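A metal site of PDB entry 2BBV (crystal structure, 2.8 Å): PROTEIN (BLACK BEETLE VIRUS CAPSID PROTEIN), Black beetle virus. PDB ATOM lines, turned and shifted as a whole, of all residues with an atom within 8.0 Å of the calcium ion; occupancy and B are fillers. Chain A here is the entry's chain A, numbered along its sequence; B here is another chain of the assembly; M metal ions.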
ATOM      1  N   THR A 216      12.502  21.722 -18.935  1.00  0.00           N
ATOM      2  CA  THR A 216      13.350  22.351 -17.920  1.00  0.00           C
ATOM      3  C   THR A 216      14.813  22.197 -18.246  1.00  0.00           C
ATOM      4  O   THR A 216      15.257  21.156 -18.747  1.00  0.00           O
ATOM      5  CB  THR A 216      13.016  21.747 -16.500  1.00  0.00           C
ATOM      6  OG1 THR A 216      13.412  22.794 -15.555  1.00  0.00           O
ATOM      7  CG2 THR A 216      13.717  20.422 -16.252  1.00  0.00           C
ATOM      8  N   LEU A 217      15.538  23.265 -17.984  1.00  0.00           N
ATOM      9  CA  LEU A 217      16.989  23.319 -18.217  1.00  0.00           C
ATOM     10  C   LEU A 217      17.656  22.756 -16.965  1.00  0.00           C
ATOM     11  O   LEU A 217      17.278  23.270 -15.875  1.00  0.00           O
ATOM     12  CB  LEU A 217      17.294  24.782 -18.483  1.00  0.00           C
ATOM     13  CG  LEU A 217      17.595  25.330 -19.856  1.00  0.00           C
ATOM     14  CD1 LEU A 217      17.346  24.357 -20.989  1.00  0.00           C
ATOM     15  CD2 LEU A 217      16.726  26.575 -20.053  1.00  0.00           C
ATOM     16  N   VAL A 218      18.546  21.786 -17.105  1.00  0.00           N
ATOM     17  CA  VAL A 218      19.256  21.227 -15.921  1.00  0.00           C
ATOM     18  C   VAL A 218      20.744  21.602 -16.062  1.00  0.00           C
ATOM     19  O   VAL A 218      21.298  21.404 -17.152  1.00  0.00           O
ATOM     20  CB  VAL A 218      19.016  19.739 -15.772  1.00  0.00           C
ATOM     21  CG1 VAL A 218      17.618  19.350 -15.388  1.00  0.00           C
ATOM     22  CG2 VAL A 218      19.449  19.011 -17.037  1.00  0.00           C
ATOM     23  N   GLY A 219      21.315  22.187 -15.026  1.00  0.00           N
ATOM     24  CA  GLY A 219      22.724  22.568 -15.108  1.00  0.00           C
ATOM     25  C   GLY A 219      22.976  24.054 -15.206  1.00  0.00           C
ATOM     26  O   GLY A 219      24.153  24.476 -15.419  1.00  0.00           O
ATOM     27  N   LEU A 220      21.947  24.847 -15.046  1.00  0.00           N
ATOM     28  CA  LEU A 220      22.046  26.314 -15.079  1.00  0.00           C
ATOM     29  C   LEU A 220      22.559  26.864 -13.749  1.00  0.00           C
ATOM     30  O   LEU A 220      22.811  28.075 -13.617  1.00  0.00           O
ATOM     31  CB  LEU A 220      20.626  26.817 -15.402  1.00  0.00           C
ATOM     32  CG  LEU A 220      20.478  27.672 -16.640  1.00  0.00           C
ATOM     33  CD1 LEU A 220      21.487  27.215 -17.708  1.00  0.00           C
ATOM     34  CD2 LEU A 220      19.070  27.517 -17.157  1.00  0.00           C
ATOM     35  N   ASP A 221      22.684  25.993 -12.762  1.00  0.00           N
ATOM     36  CA  ASP A 221      23.141  26.397 -11.406  1.00  0.00           C
ATOM     37  C   ASP A 221      24.660  26.636 -11.459  1.00  0.00           C
ATOM     38  O   ASP A 221      25.290  27.112 -10.509  1.00  0.00           O
ATOM     39  CB  ASP A 221      22.725  25.337 -10.391  1.00  0.00           C
ATOM     40  CG  ASP A 221      21.318  25.525  -9.842  1.00  0.00           C
ATOM     41  OD1 ASP A 221      20.971  26.626  -9.364  1.00  0.00           O
ATOM     42  OD2 ASP A 221      20.527  24.541  -9.880  1.00  0.00           O
ATOM     43  N   GLY A 222      25.191  26.270 -12.606  1.00  0.00           N
ATOM     44  CA  GLY A 222      26.602  26.371 -12.921  1.00  0.00           C
ATOM     45  C   GLY A 222      26.929  27.815 -13.245  1.00  0.00           C
ATOM     46  O   GLY A 222      28.109  28.209 -13.149  1.00  0.00           O
ATOM     47  N   LEU A 224      26.046  30.255 -11.536  1.00  0.00           N
ATOM     48  CA  LEU A 224      26.079  30.879 -10.224  1.00  0.00           C
ATOM     49  C   LEU A 224      27.399  30.984  -9.530  1.00  0.00           C
ATOM     50  O   LEU A 224      27.442  31.527  -8.380  1.00  0.00           O
ATOM     51  CB  LEU A 224      25.016  30.122  -9.387  1.00  0.00           C
ATOM     52  CG  LEU A 224      23.604  30.270  -9.947  1.00  0.00           C
ATOM     53  CD1 LEU A 224      22.562  29.659  -9.058  1.00  0.00           C
ATOM     54  CD2 LEU A 224      23.364  31.754 -10.151  1.00  0.00           C
ATOM     55  N   VAL A 269       9.303  29.767 -11.429  1.00  0.00           N
ATOM     56  CA  VAL A 269      10.715  29.465 -11.544  1.00  0.00           C
ATOM     57  C   VAL A 269      11.070  28.419 -10.479  1.00  0.00           C
ATOM     58  O   VAL A 269      12.031  27.655 -10.630  1.00  0.00           O
ATOM     59  CB  VAL A 269      11.541  30.724 -11.319  1.00  0.00           C
ATOM     60  CG1 VAL A 269      12.911  30.439 -10.690  1.00  0.00           C
ATOM     61  CG2 VAL A 269      11.829  31.494 -12.616  1.00  0.00           C
ATOM     62  N   ALA A 270      10.275  28.415  -9.420  1.00  0.00           N
ATOM     63  CA  ALA A 270      10.507  27.518  -8.266  1.00  0.00           C
ATOM     64  C   ALA A 270      10.127  26.062  -8.556  1.00  0.00           C
ATOM     65  O   ALA A 270      10.733  25.118  -8.045  1.00  0.00           O
ATOM     66  CB  ALA A 270       9.697  27.976  -7.053  1.00  0.00           C
ATOM     67  N   SER A 272      10.090  24.744 -11.618  1.00  0.00           N
ATOM     68  CA  SER A 272      10.949  24.338 -12.742  1.00  0.00           C
ATOM     69  C   SER A 272      12.273  23.810 -12.209  1.00  0.00           C
ATOM     70  O   SER A 272      12.906  22.912 -12.791  1.00  0.00           O
ATOM     71  CB  SER A 272      11.229  25.528 -13.648  1.00  0.00           C
ATOM     72  OG  SER A 272      12.221  26.367 -13.051  1.00  0.00           O
ATOM     73  N   GLY A 273      12.668  24.389 -11.095  1.00  0.00           N
ATOM     74  CA  GLY A 273      13.925  24.052 -10.435  1.00  0.00           C
ATOM     75  C   GLY A 273      15.097  24.760 -11.126  1.00  0.00           C
ATOM     76  O   GLY A 273      16.252  24.349 -10.984  1.00  0.00           O
ATOM     77  N   GLN A 274      14.768  25.809 -11.869  1.00  0.00           N
ATOM     78  CA  GLN A 274      15.771  26.635 -12.578  1.00  0.00           C
ATOM     79  C   GLN A 274      16.156  27.842 -11.731  1.00  0.00           C
ATOM     80  O   GLN A 274      15.294  28.472 -11.084  1.00  0.00           O
ATOM     81  CB  GLN A 274      15.208  27.155 -13.899  1.00  0.00           C
ATOM     82  CG  GLN A 274      15.088  26.058 -14.961  1.00  0.00           C
ATOM     83  CD  GLN A 274      14.788  26.602 -16.359  1.00  0.00           C
ATOM     84  OE1 GLN A 274      15.225  27.697 -16.698  1.00  0.00           O
ATOM     85  NE2 GLN A 274      14.057  25.891 -17.197  1.00  0.00           N
ATOM     86  N   PRO A 275      17.445  28.211 -11.690  1.00  0.00           N
ATOM     87  CA  PRO A 275      17.915  29.338 -10.908  1.00  0.00           C
ATOM     88  C   PRO A 275      17.394  30.627 -11.479  1.00  0.00           C
ATOM     89  O   PRO A 275      17.293  31.639 -10.736  1.00  0.00           O
ATOM     90  CB  PRO A 275      19.403  29.349 -11.068  1.00  0.00           C
ATOM     91  CG  PRO A 275      19.762  28.241 -12.036  1.00  0.00           C
ATOM     92  CD  PRO A 275      18.503  27.517 -12.421  1.00  0.00           C
ATOM     93  N   PHE A 276      17.119  30.612 -12.780  1.00  0.00           N
ATOM     94  CA  PHE A 276      16.592  31.818 -13.419  1.00  0.00           C
ATOM     95  C   PHE A 276      15.720  31.488 -14.639  1.00  0.00           C
ATOM     96  O   PHE A 276      15.290  30.334 -14.815  1.00  0.00           O
ATOM     97  CB  PHE A 276      17.710  32.806 -13.805  1.00  0.00           C
ATOM     98  CG  PHE A 276      19.009  32.166 -14.267  1.00  0.00           C
ATOM     99  CD1 PHE A 276      20.011  31.849 -13.342  1.00  0.00           C
ATOM    100  CD2 PHE A 276      19.218  31.931 -15.631  1.00  0.00           C
ATOM    101  CE1 PHE A 276      21.216  31.288 -13.781  1.00  0.00           C
ATOM    102  CE2 PHE A 276      20.414  31.375 -16.066  1.00  0.00           C
ATOM    103  CZ  PHE A 276      21.419  31.045 -15.146  1.00  0.00           C
ATOM    104  N   ALA B 157      12.728  19.223  -6.708  1.00  0.00           N
ATOM    105  CA  ALA B 157      13.218  19.918  -7.918  1.00  0.00           C
ATOM    106  C   ALA B 157      14.625  20.436  -7.757  1.00  0.00           C
ATOM    107  O   ALA B 157      14.995  21.445  -8.410  1.00  0.00           O
ATOM    108  CB  ALA B 157      12.202  20.921  -8.388  1.00  0.00           C
ATOM    109  N   SER B 158      15.448  19.771  -6.952  1.00  0.00           N
ATOM    110  CA  SER B 158      16.847  20.235  -6.795  1.00  0.00           C
ATOM    111  C   SER B 158      17.804  19.112  -7.180  1.00  0.00           C
ATOM    112  O   SER B 158      18.936  19.070  -6.649  1.00  0.00           O
ATOM    113  CB  SER B 158      17.148  20.656  -5.372  1.00  0.00           C
ATOM    114  OG  SER B 158      16.234  21.611  -4.889  1.00  0.00           O
ATOM    115  N   ARG B 159      17.303  18.241  -8.057  1.00  0.00           N
ATOM    116  CA  ARG B 159      18.097  17.077  -8.447  1.00  0.00           C
ATOM    117  C   ARG B 159      19.381  17.423  -9.159  1.00  0.00           C
ATOM    118  O   ARG B 159      20.415  16.732  -8.925  1.00  0.00           O
ATOM    119  CB  ARG B 159      17.271  16.044  -9.171  1.00  0.00           C
ATOM    120  CG  ARG B 159      16.388  15.216  -8.271  1.00  0.00           C
ATOM    121  CD  ARG B 159      16.573  15.431  -6.800  1.00  0.00           C
ATOM    122  NE  ARG B 159      15.540  14.723  -6.033  1.00  0.00           N
ATOM    123  CZ  ARG B 159      15.455  14.755  -4.698  1.00  0.00           C
ATOM    124  NH1 ARG B 159      16.371  15.415  -3.980  1.00  0.00           N
ATOM    125  NH2 ARG B 159      14.486  14.125  -4.015  1.00  0.00           N
ATOM    126  N   SER B 160      19.393  18.480  -9.955  1.00  0.00           N
ATOM    127  CA  SER B 160      20.590  18.860 -10.705  1.00  0.00           C
ATOM    128  C   SER B 160      21.393  20.015 -10.187  1.00  0.00           C
ATOM    129  O   SER B 160      22.020  20.700 -11.039  1.00  0.00           O
ATOM    130  CB  SER B 160      20.248  19.096 -12.167  1.00  0.00           C
ATOM    131  OG  SER B 160      18.892  19.456 -12.327  1.00  0.00           O
ATOM    132  N   ASP B 161      21.410  20.250  -8.897  1.00  0.00           N
ATOM    133  CA  ASP B 161      22.213  21.404  -8.379  1.00  0.00           C
ATOM    134  C   ASP B 161      23.685  21.084  -8.553  1.00  0.00           C
ATOM    135  O   ASP B 161      24.399  21.931  -9.138  1.00  0.00           O
ATOM    136  CB  ASP B 161      21.759  21.813  -7.001  1.00  0.00           C
ATOM    137  CG  ASP B 161      20.478  22.612  -6.977  1.00  0.00           C
ATOM    138  OD1 ASP B 161      19.810  22.717  -8.046  1.00  0.00           O
ATOM    139  OD2 ASP B 161      20.052  23.163  -5.947  1.00  0.00           O
ATOM    140  N   GLN B 162      24.109  19.907  -8.123  1.00  0.00           N
ATOM    141  CA  GLN B 162      25.464  19.409  -8.184  1.00  0.00           C
ATOM    142  C   GLN B 162      25.911  18.912  -9.578  1.00  0.00           C
ATOM    143  O   GLN B 162      26.994  19.265 -10.101  1.00  0.00           O
ATOM    144  CB  GLN B 162      25.724  18.236  -7.239  1.00  0.00           C
ATOM    145  CG  GLN B 162      25.701  18.482  -5.745  1.00  0.00           C
ATOM    146  CD  GLN B 162      26.265  19.845  -5.435  1.00  0.00           C
ATOM    147  OE1 GLN B 162      27.466  20.056  -5.492  1.00  0.00           O
ATOM    148  NE2 GLN B 162      25.361  20.756  -5.134  1.00  0.00           N
ATOM    149  N   GLU B 257      13.806  15.975 -12.973  1.00  0.00           N
ATOM    150  CA  GLU B 257      13.322  16.737 -11.823  1.00  0.00           C
ATOM    151  C   GLU B 257      11.890  16.439 -11.432  1.00  0.00           C
ATOM    152  O   GLU B 257      11.038  16.306 -12.331  1.00  0.00           O
ATOM    153  CB  GLU B 257      13.425  18.241 -12.186  1.00  0.00           C
ATOM    154  CG  GLU B 257      14.901  18.648 -12.336  1.00  0.00           C
ATOM    155  CD  GLU B 257      15.591  18.806 -11.014  1.00  0.00           C
ATOM    156  OE1 GLU B 257      14.922  18.383 -10.064  1.00  0.00           O
ATOM    157  OE2 GLU B 257      16.680  19.320 -10.861  1.00  0.00           O
ATOM    158  N   ASN B 324      28.725  20.188 -12.301  1.00  0.00           N
ATOM    159  CA  ASN B 324      28.324  21.592 -12.489  1.00  0.00           C
ATOM    160  C   ASN B 324      29.444  22.429 -11.835  1.00  0.00           C
ATOM    161  O   ASN B 324      29.801  22.105 -10.692  1.00  0.00           O
ATOM    162  CB  ASN B 324      26.995  21.867 -11.782  1.00  0.00           C
ATOM    163  CG  ASN B 324      25.783  21.489 -12.632  1.00  0.00           C
ATOM    164  OD1 ASN B 324      24.876  20.808 -12.139  1.00  0.00           O
ATOM    165  ND2 ASN B 324      25.702  21.892 -13.883  1.00  0.00           N
ATOM    166  N   ASN B 326      29.479  25.012 -10.323  1.00  0.00           N
ATOM    167  CA  ASN B 326      29.097  25.563  -9.032  1.00  0.00           C
ATOM    168  C   ASN B 326      29.165  24.511  -7.909  1.00  0.00           C
ATOM    169  O   ASN B 326      29.264  24.933  -6.738  1.00  0.00           O
ATOM    170  CB  ASN B 326      27.654  26.080  -9.069  1.00  0.00           C
ATOM    171  CG  ASN B 326      26.682  24.925  -9.301  1.00  0.00           C
ATOM    172  OD1 ASN B 326      25.880  24.570  -8.440  1.00  0.00           O
ATOM    173  ND2 ASN B 326      26.777  24.338 -10.499  1.00  0.00           N
HETATM  174 CA    CA M   1      18.223  23.820  -9.936  1.00  0.00          CA
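The backbone carbonyl oxygen of Asp 221 lies close to the side-chain amide nitrogen of Asn 326 of chain B (3.1 Å).
The backbone carbonyl oxygen (O) of Asp 161 of chain B sits close to the side-chain amide oxygen (OD1) of Asn 324 of chain B.
OD1 of Asn 326 of chain B lies close to O of Asp 161 of chain B (3.1 Å).
Of the 24 residues printed, 3 come within 4 Å of the calcium ion.
The calcium ion is bound by the backbone carbonyl oxygen (O) of Gly 273 (2.3 Å).
The calcium ion is bound by OD2 of Asp 221, at 2.4 Å.
OD1 of Asp 161 of chain B is bound to the calcium ion (2.7 Å).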
